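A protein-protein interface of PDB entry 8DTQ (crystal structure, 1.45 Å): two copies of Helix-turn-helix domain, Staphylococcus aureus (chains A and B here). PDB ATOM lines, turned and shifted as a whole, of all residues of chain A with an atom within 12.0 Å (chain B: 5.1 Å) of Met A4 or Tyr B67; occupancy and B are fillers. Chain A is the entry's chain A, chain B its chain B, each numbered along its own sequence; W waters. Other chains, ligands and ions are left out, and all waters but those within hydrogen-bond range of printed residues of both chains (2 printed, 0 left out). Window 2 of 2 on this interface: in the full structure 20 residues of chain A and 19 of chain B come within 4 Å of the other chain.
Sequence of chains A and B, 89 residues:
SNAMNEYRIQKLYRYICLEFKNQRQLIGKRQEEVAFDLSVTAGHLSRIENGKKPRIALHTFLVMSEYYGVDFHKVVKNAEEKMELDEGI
The backbone NH of Asn A5 sits at hydrogen-bond distance from the side-chain carboxylate of Glu B66 (3.3 Å).
Of the printed residues of chain B, Met A4 touches Val B63, Glu B66 and Tyr B67.
Glu A6 touches none of the printed residues of chain B.
Of the printed residues of chain B, Ile A9 touches Leu B62, Val B63 and Glu B66.
Lys A11 touches none of the printed residues of chain B.
Printed residues of chain B within 4 Å of Leu A12: Leu B62.
No residue of chain A comes within 4 Å of Asp B37.
No residue of chain A comes within 4 Å of Leu B38.
Of chain A, only Met A4 comes within 4 Å of Tyr B67.
No residue of chain A comes within 4 Å of Tyr B68.
No residue of chain A comes within 4 Å of Gly B69.
The nearest printed residue of chain B that does not touch Ile A9 is Met B64 (6.1 Å).
No position is printed for both chains.
Met A4 touches Val B63 (CE to O, 3.2 Å).
CG of Glu B66 touches CE of Met A4, 3.7 Å away.
Tyr B67 touches Met A4.
Ile A9 touches Leu B62.
Ile A9 touches Val B63.
CB of Glu B66 touches CD1 of Ile A9, 3.9 Å away.
Leu B62 touches Leu A12.
The side-chain amide oxygen (OD1) of Asn A5 lies within hydrogen-bond range of the backbone NH (N) of Arg A8.
The side-chain amino group of Lys B29 lies within hydrogen-bond range of the side-chain hydroxyl of Tyr B67, 3.2 Å away.
The side-chain carboxylate of Asp B37 sits at hydrogen-bond distance from the side-chain hydroxyl of Tyr B67 (2.6 Å).
Water W2 lies within hydrogen-bond range of OE1 of Glu B66 (2.8 Å) and NH1 of Arg A8 (2.9 Å).
Water W1 lies within hydrogen-bond range of the side-chain carboxylate (OE1) of Glu B66 (2.9 Å) and the side-chain amide nitrogen (ND2) of Asn A5 (3.1 Å).
Hydrophobic or aromatic side chains of chain B that line the printed part of chain A: Leu B62 and Val B63.
Among the printed residues, no Asp or Glu carboxylate lies within 4 Å of a Lys or Arg side-chain nitrogen of the other chain.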
ATOM      1  N   MET A   4     -13.349 -10.219  20.311  1.00  0.00           N
ATOM      2  CA  MET A   4     -13.918 -11.192  19.381  1.00  0.00           C
ATOM      3  C   MET A   4     -15.439 -11.235  19.467  1.00  0.00           C
ATOM      4  O   MET A   4     -16.012 -11.381  20.545  1.00  0.00           O
ATOM      5  CB  MET A   4     -13.340 -12.587  19.631  1.00  0.00           C
ATOM      6  CG  MET A   4     -11.863 -12.736  19.281  1.00  0.00           C
ATOM      7  SD  MET A   4     -11.516 -12.618  17.350  1.00  0.00           S
ATOM      8  CE  MET A   4     -12.230 -14.335  16.807  1.00  0.00           C
ATOM      9  N   ASN A   5     -16.096 -11.119  18.314  1.00  0.00           N
ATOM     10  CA  ASN A   5     -17.553 -11.020  18.262  1.00  0.00           C
ATOM     11  C   ASN A   5     -18.141 -12.431  18.244  1.00  0.00           C
ATOM     12  O   ASN A   5     -18.508 -12.979  17.198  1.00  0.00           O
ATOM     13  CB  ASN A   5     -17.965 -10.212  17.039  1.00  0.00           C
ATOM     14  CG  ASN A   5     -19.403  -9.772  17.090  1.00  0.00           C
ATOM     15  OD1 ASN A   5     -20.234 -10.377  17.790  1.00  0.00           O
ATOM     16  ND2 ASN A   5     -19.720  -8.705  16.339  1.00  0.00           N
ATOM     17  N   GLU A   6     -18.259 -13.012  19.446  1.00  0.00           N
ATOM     18  CA  GLU A   6     -18.778 -14.376  19.569  1.00  0.00           C
ATOM     19  C   GLU A   6     -20.244 -14.457  19.171  1.00  0.00           C
ATOM     20  O   GLU A   6     -20.673 -15.450  18.568  1.00  0.00           O
ATOM     21  CB  GLU A   6     -18.629 -14.856  21.011  1.00  0.00           C
ATOM     22  N   TYR A   7     -21.015 -13.408  19.453  1.00  0.00           N
ATOM     23  CA  TYR A   7     -22.417 -13.405  19.064  1.00  0.00           C
ATOM     24  C   TYR A   7     -22.553 -13.548  17.556  1.00  0.00           C
ATOM     25  O   TYR A   7     -23.345 -14.366  17.064  1.00  0.00           O
ATOM     26  CB  TYR A   7     -23.074 -12.105  19.547  1.00  0.00           C
ATOM     27  CG  TYR A   7     -24.530 -11.997  19.193  1.00  0.00           C
ATOM     28  CD1 TYR A   7     -25.515 -12.450  20.064  1.00  0.00           C
ATOM     29  CD2 TYR A   7     -24.927 -11.457  17.981  1.00  0.00           C
ATOM     30  CE1 TYR A   7     -26.849 -12.355  19.740  1.00  0.00           C
ATOM     31  CE2 TYR A   7     -26.248 -11.366  17.644  1.00  0.00           C
ATOM     32  CZ  TYR A   7     -27.210 -11.814  18.529  1.00  0.00           C
ATOM     33  OH  TYR A   7     -28.536 -11.717  18.198  1.00  0.00           O
ATOM     34  N   ARG A   8     -21.776 -12.758  16.802  1.00  0.00           N
ATOM     35  CA  ARG A   8     -21.864 -12.809  15.351  1.00  0.00           C
ATOM     36  C   ARG A   8     -21.377 -14.135  14.794  1.00  0.00           C
ATOM     37  O   ARG A   8     -21.972 -14.663  13.845  1.00  0.00           O
ATOM     38  CB  ARG A   8     -21.061 -11.659  14.748  1.00  0.00           C
ATOM     39  CG  ARG A   8     -21.471 -11.356  13.329  1.00  0.00           C
ATOM     40  CD  ARG A   8     -20.669 -10.229  12.700  1.00  0.00           C
ATOM     41  NE  ARG A   8     -20.998 -10.079  11.280  1.00  0.00           N
ATOM     42  CZ  ARG A   8     -20.415 -10.711  10.269  1.00  0.00           C
ATOM     43  NH1 ARG A   8     -19.445 -11.595  10.465  1.00  0.00           N
ATOM     44  NH2 ARG A   8     -20.831 -10.465   9.027  1.00  0.00           N
ATOM     45  N   ILE A   9     -20.278 -14.671  15.348  1.00  0.00           N
ATOM     46  CA  ILE A   9     -19.754 -15.960  14.892  1.00  0.00           C
ATOM     47  C   ILE A   9     -20.810 -17.043  15.017  1.00  0.00           C
ATOM     48  O   ILE A   9     -21.005 -17.854  14.108  1.00  0.00           O
ATOM     49  CB  ILE A   9     -18.474 -16.341  15.669  1.00  0.00           C
ATOM     50  CG1 ILE A   9     -17.310 -15.411  15.283  1.00  0.00           C
ATOM     51  CG2 ILE A   9     -18.131 -17.822  15.454  1.00  0.00           C
ATOM     52  CD1 ILE A   9     -16.172 -15.435  16.270  1.00  0.00           C
ATOM     53  N   GLN A  10     -21.505 -17.078  16.147  1.00  0.00           N
ATOM     54  CA  GLN A  10     -22.490 -18.127  16.365  1.00  0.00           C
ATOM     55  C   GLN A  10     -23.733 -17.911  15.502  1.00  0.00           C
ATOM     56  O   GLN A  10     -24.272 -18.866  14.929  1.00  0.00           O
ATOM     57  CB  GLN A  10     -22.848 -18.173  17.848  1.00  0.00           C
ATOM     58  CG  GLN A  10     -23.433 -19.488  18.311  1.00  0.00           C
ATOM     59  CD  GLN A  10     -24.915 -19.550  18.067  1.00  0.00           C
ATOM     60  OE1 GLN A  10     -25.606 -18.529  18.122  1.00  0.00           O
ATOM     61  NE2 GLN A  10     -25.423 -20.756  17.820  1.00  0.00           N
ATOM     62  N   LYS A  11     -24.206 -16.665  15.384  1.00  0.00           N
ATOM     63  CA  LYS A  11     -25.370 -16.428  14.532  1.00  0.00           C
ATOM     64  C   LYS A  11     -25.064 -16.743  13.074  1.00  0.00           C
ATOM     65  O   LYS A  11     -25.901 -17.315  12.367  1.00  0.00           O
ATOM     66  CB  LYS A  11     -25.838 -14.976  14.655  1.00  0.00           C
ATOM     67  CG  LYS A  11     -26.517 -14.666  15.972  1.00  0.00           C
ATOM     68  CD  LYS A  11     -27.850 -15.371  16.091  1.00  0.00           C
ATOM     69  CE  LYS A  11     -28.480 -15.048  17.435  1.00  0.00           C
ATOM     70  NZ  LYS A  11     -29.758 -15.749  17.587  1.00  0.00           N
ATOM     71  N   LEU A  12     -23.890 -16.331  12.586  1.00  0.00           N
ATOM     72  CA  LEU A  12     -23.579 -16.583  11.188  1.00  0.00           C
ATOM     73  C   LEU A  12     -23.543 -18.082  10.909  1.00  0.00           C
ATOM     74  O   LEU A  12     -24.055 -18.539   9.881  1.00  0.00           O
ATOM     75  CB  LEU A  12     -22.254 -15.908  10.829  1.00  0.00           C
ATOM     76  CG  LEU A  12     -21.745 -16.156   9.404  1.00  0.00           C
ATOM     77  CD1 LEU A  12     -22.795 -15.740   8.369  1.00  0.00           C
ATOM     78  CD2 LEU A  12     -20.450 -15.386   9.179  1.00  0.00           C
ATOM     79  N   ARG A  55     -20.553 -27.718  15.929  1.00  0.00           N
ATOM     80  CA  ARG A  55     -19.174 -28.020  15.555  1.00  0.00           C
ATOM     81  C   ARG A  55     -19.085 -28.902  14.311  1.00  0.00           C
ATOM     82  O   ARG A  55     -18.131 -29.676  14.140  1.00  0.00           O
ATOM     83  CB  ARG A  55     -18.391 -28.605  16.726  1.00  0.00           C
ATOM     84  CG  ARG A  55     -18.119 -27.613  17.856  1.00  0.00           C
ATOM     85  CD  ARG A  55     -17.783 -26.207  17.368  1.00  0.00           C
ATOM     86  NE  ARG A  55     -17.293 -25.376  18.461  1.00  0.00           N
ATOM     87  CZ  ARG A  55     -17.864 -24.257  18.891  1.00  0.00           C
ATOM     88  NH1 ARG A  55     -17.359 -23.573  19.906  1.00  0.00           N
ATOM     89  NH2 ARG A  55     -18.969 -23.815  18.293  1.00  0.00           N
ATOM     90  N   GLU A  80     -24.686 -14.277   5.282  1.00  0.00           N
ATOM     91  CA  GLU A  80     -24.223 -13.014   5.845  1.00  0.00           C
ATOM     92  C   GLU A  80     -25.238 -11.910   5.596  1.00  0.00           C
ATOM     93  O   GLU A  80     -25.543 -11.109   6.496  1.00  0.00           O
ATOM     94  CB  GLU A  80     -22.882 -12.619   5.220  1.00  0.00           C
ATOM     95  CG  GLU A  80     -21.711 -13.559   5.514  1.00  0.00           C
ATOM     96  CD  GLU A  80     -20.508 -13.278   4.635  1.00  0.00           C
ATOM     97  OE1 GLU A  80     -20.609 -12.407   3.734  1.00  0.00           O
ATOM     98  OE2 GLU A  80     -19.463 -13.927   4.844  1.00  0.00           O
ATOM     99  N   ILE A  89     -26.017  -6.804  11.851  1.00  0.00           N
ATOM    100  CA  ILE A  89     -24.607  -7.072  12.101  1.00  0.00           C
ATOM    101  C   ILE A  89     -24.002  -7.880  10.962  1.00  0.00           C
ATOM    102  O   ILE A  89     -24.741  -8.409  10.130  1.00  0.00           O
ATOM    103  CB  ILE A  89     -24.394  -7.787  13.444  1.00  0.00           C
ATOM    104  CG1 ILE A  89     -25.028  -9.189  13.407  1.00  0.00           C
ATOM    105  CG2 ILE A  89     -24.949  -6.923  14.602  1.00  0.00           C
ATOM    106  CD1 ILE A  89     -24.804 -10.018  14.675  1.00  0.00           C
ATOM    107  OXT ILE A  89     -22.775  -8.037  10.867  1.00  0.00           O
ATOM    108  N   LYS B  29       2.168 -11.258  10.277  1.00  0.00           N
ATOM    109  CA  LYS B  29       2.185 -11.838  11.614  1.00  0.00           C
ATOM    110  C   LYS B  29       2.741 -13.255  11.585  1.00  0.00           C
ATOM    111  O   LYS B  29       2.539 -13.998  10.618  1.00  0.00           O
ATOM    112  CB  LYS B  29       0.783 -11.823  12.234  1.00  0.00           C
ATOM    113  CG  LYS B  29       0.402 -10.457  12.805  1.00  0.00           C
ATOM    114  CD  LYS B  29      -1.081 -10.376  13.132  1.00  0.00           C
ATOM    115  CE  LYS B  29      -1.437  -9.065  13.832  1.00  0.00           C
ATOM    116  NZ  LYS B  29      -2.846  -9.055  14.351  1.00  0.00           N
ATOM    117  N   GLU B  33       2.103 -15.465  17.044  1.00  0.00           N
ATOM    118  CA  GLU B  33       1.328 -14.308  17.477  1.00  0.00           C
ATOM    119  C   GLU B  33      -0.167 -14.539  17.278  1.00  0.00           C
ATOM    120  O   GLU B  33      -0.972 -14.298  18.186  1.00  0.00           O
ATOM    121  CB  GLU B  33       1.790 -13.052  16.744  1.00  0.00           C
ATOM    122  CG  GLU B  33       0.826 -11.898  16.895  1.00  0.00           C
ATOM    123  CD  GLU B  33       1.407 -10.571  16.437  1.00  0.00           C
ATOM    124  OE1 GLU B  33       2.443 -10.570  15.724  1.00  0.00           O
ATOM    125  OE2 GLU B  33       0.816  -9.524  16.789  1.00  0.00           O
ATOM    126  N   VAL B  34      -0.556 -15.017  16.097  1.00  0.00           N
ATOM    127  CA  VAL B  34      -1.966 -15.274  15.831  1.00  0.00           C
ATOM    128  C   VAL B  34      -2.483 -16.375  16.744  1.00  0.00           C
ATOM    129  O   VAL B  34      -3.584 -16.276  17.297  1.00  0.00           O
ATOM    130  CB  VAL B  34      -2.196 -15.605  14.342  1.00  0.00           C
ATOM    131  CG1 VAL B  34      -3.671 -15.981  14.111  1.00  0.00           C
ATOM    132  CG2 VAL B  34      -1.791 -14.433  13.459  1.00  0.00           C
ATOM    133  N   ASP B  37      -3.294 -15.002  20.104  1.00  0.00           N
ATOM    134  CA  ASP B  37      -4.533 -14.235  20.060  1.00  0.00           C
ATOM    135  C   ASP B  37      -5.763 -15.136  20.044  1.00  0.00           C
ATOM    136  O   ASP B  37      -6.814 -14.765  20.590  1.00  0.00           O
ATOM    137  CB  ASP B  37      -4.553 -13.332  18.826  1.00  0.00           C
ATOM    138  CG  ASP B  37      -3.583 -12.169  18.921  1.00  0.00           C
ATOM    139  OD1 ASP B  37      -3.023 -11.926  20.013  1.00  0.00           O
ATOM    140  OD2 ASP B  37      -3.400 -11.485  17.893  1.00  0.00           O
ATOM    141  N   LEU B  38      -5.670 -16.294  19.393  1.00  0.00           N
ATOM    142  CA  LEU B  38      -6.779 -17.230  19.252  1.00  0.00           C
ATOM    143  C   LEU B  38      -6.825 -18.286  20.349  1.00  0.00           C
ATOM    144  O   LEU B  38      -7.711 -19.146  20.313  1.00  0.00           O
ATOM    145  CB  LEU B  38      -6.710 -17.922  17.888  1.00  0.00           C
ATOM    146  CG  LEU B  38      -6.824 -16.994  16.680  1.00  0.00           C
ATOM    147  CD1 LEU B  38      -6.687 -17.781  15.383  1.00  0.00           C
ATOM    148  CD2 LEU B  38      -8.160 -16.258  16.724  1.00  0.00           C
ATOM    149  N   LEU B  62     -14.938 -19.556  10.931  1.00  0.00           N
ATOM    150  CA  LEU B  62     -15.631 -18.302  11.220  1.00  0.00           C
ATOM    151  C   LEU B  62     -14.892 -17.470  12.267  1.00  0.00           C
ATOM    152  O   LEU B  62     -14.869 -16.228  12.178  1.00  0.00           O
ATOM    153  CB  LEU B  62     -17.071 -18.587  11.627  1.00  0.00           C
ATOM    154  CG  LEU B  62     -17.931 -19.276  10.565  1.00  0.00           C
ATOM    155  CD1 LEU B  62     -19.344 -19.507  11.089  1.00  0.00           C
ATOM    156  CD2 LEU B  62     -17.999 -18.414   9.293  1.00  0.00           C
ATOM    157  N   VAL B  63     -14.313 -18.122  13.281  1.00  0.00           N
ATOM    158  CA  VAL B  63     -13.491 -17.412  14.260  1.00  0.00           C
ATOM    159  C   VAL B  63     -12.323 -16.722  13.556  1.00  0.00           C
ATOM    160  O   VAL B  63     -12.009 -15.555  13.820  1.00  0.00           O
ATOM    161  CB  VAL B  63     -12.988 -18.383  15.345  1.00  0.00           C
ATOM    162  CG1 VAL B  63     -11.939 -17.722  16.208  1.00  0.00           C
ATOM    163  CG2 VAL B  63     -14.155 -18.920  16.209  1.00  0.00           C
ATOM    164  N   MET B  64     -11.665 -17.430  12.655  1.00  0.00           N
ATOM    165  CA  MET B  64     -10.514 -16.857  11.968  1.00  0.00           C
ATOM    166  C   MET B  64     -10.927 -15.700  11.047  1.00  0.00           C
ATOM    167  O   MET B  64     -10.209 -14.687  10.943  1.00  0.00           O
ATOM    168  CB  MET B  64      -9.743 -17.947  11.222  1.00  0.00           C
ATOM    169  CG  MET B  64      -9.166 -19.009  12.181  1.00  0.00           C
ATOM    170  SD  MET B  64      -8.519 -20.612  11.305  1.00  0.00           S
ATOM    171  CE  MET B  64      -6.924 -19.916  10.388  1.00  0.00           C
ATOM    172  N   SER B  65     -12.078 -15.832  10.373  1.00  0.00           N
ATOM    173  CA  SER B  65     -12.567 -14.724   9.536  1.00  0.00           C
ATOM    174  C   SER B  65     -12.818 -13.489  10.390  1.00  0.00           C
ATOM    175  O   SER B  65     -12.509 -12.364   9.991  1.00  0.00           O
ATOM    176  CB  SER B  65     -13.867 -15.112   8.832  1.00  0.00           C
ATOM    177  OG  SER B  65     -13.667 -16.080   7.825  1.00  0.00           O
ATOM    178  N   GLU B  66     -13.391 -13.681  11.573  1.00  0.00           N
ATOM    179  CA  GLU B  66     -13.610 -12.559  12.479  1.00  0.00           C
ATOM    180  C   GLU B  66     -12.279 -11.967  12.929  1.00  0.00           C
ATOM    181  O   GLU B  66     -12.102 -10.740  12.960  1.00  0.00           O
ATOM    182  CB  GLU B  66     -14.441 -13.054  13.664  1.00  0.00           C
ATOM    183  CG  GLU B  66     -14.500 -12.131  14.862  1.00  0.00           C
ATOM    184  CD  GLU B  66     -15.302 -10.885  14.617  1.00  0.00           C
ATOM    185  OE1 GLU B  66     -16.087 -10.851  13.637  1.00  0.00           O
ATOM    186  OE2 GLU B  66     -15.131  -9.935  15.422  1.00  0.00           O
ATOM    187  N   TYR B  67     -11.312 -12.826  13.226  1.00  0.00           N
ATOM    188  CA  TYR B  67     -10.013 -12.354  13.688  1.00  0.00           C
ATOM    189  C   TYR B  67      -9.336 -11.483  12.641  1.00  0.00           C
ATOM    190  O   TYR B  67      -8.800 -10.415  12.958  1.00  0.00           O
ATOM    191  CB  TYR B  67      -9.119 -13.532  14.063  1.00  0.00           C
ATOM    192  CG  TYR B  67      -7.725 -13.100  14.416  1.00  0.00           C
ATOM    193  CD1 TYR B  67      -7.435 -12.557  15.666  1.00  0.00           C
ATOM    194  CD2 TYR B  67      -6.675 -13.273  13.514  1.00  0.00           C
ATOM    195  CE1 TYR B  67      -6.152 -12.155  15.993  1.00  0.00           C
ATOM    196  CE2 TYR B  67      -5.383 -12.890  13.836  1.00  0.00           C
ATOM    197  CZ  TYR B  67      -5.123 -12.329  15.073  1.00  0.00           C
ATOM    198  OH  TYR B  67      -3.829 -11.955  15.384  1.00  0.00           O
ATOM    199  N   TYR B  68      -9.354 -11.923  11.384  1.00  0.00           N
ATOM    200  CA  TYR B  68      -8.730 -11.163  10.308  1.00  0.00           C
ATOM    201  C   TYR B  68      -9.610 -10.040   9.798  1.00  0.00           C
ATOM    202  O   TYR B  68      -9.121  -9.193   9.047  1.00  0.00           O
ATOM    203  CB  TYR B  68      -8.337 -12.084   9.146  1.00  0.00           C
ATOM    204  CG  TYR B  68      -7.203 -13.024   9.502  1.00  0.00           C
ATOM    205  CD1 TYR B  68      -5.946 -12.532   9.855  1.00  0.00           C
ATOM    206  CD2 TYR B  68      -7.402 -14.403   9.557  1.00  0.00           C
ATOM    207  CE1 TYR B  68      -4.917 -13.381  10.205  1.00  0.00           C
ATOM    208  CE2 TYR B  68      -6.359 -15.265   9.902  1.00  0.00           C
ATOM    209  CZ  TYR B  68      -5.130 -14.744  10.237  1.00  0.00           C
ATOM    210  OH  TYR B  68      -4.102 -15.579  10.583  1.00  0.00           O
ATOM    211  N   GLY B  69     -10.881 -10.011  10.184  1.00  0.00           N
ATOM    212  CA  GLY B  69     -11.770  -8.969   9.707  1.00  0.00           C
ATOM    213  C   GLY B  69     -12.109  -9.072   8.236  1.00  0.00           C
ATOM    214  O   GLY B  69     -12.346  -8.048   7.594  1.00  0.00           O
HETATM  215  O   HOH W   1     -17.478  -8.358  14.228  1.00  0.00           O
HETATM  216  O   HOH W   2     -18.087 -12.565  12.791  1.00  0.00           O
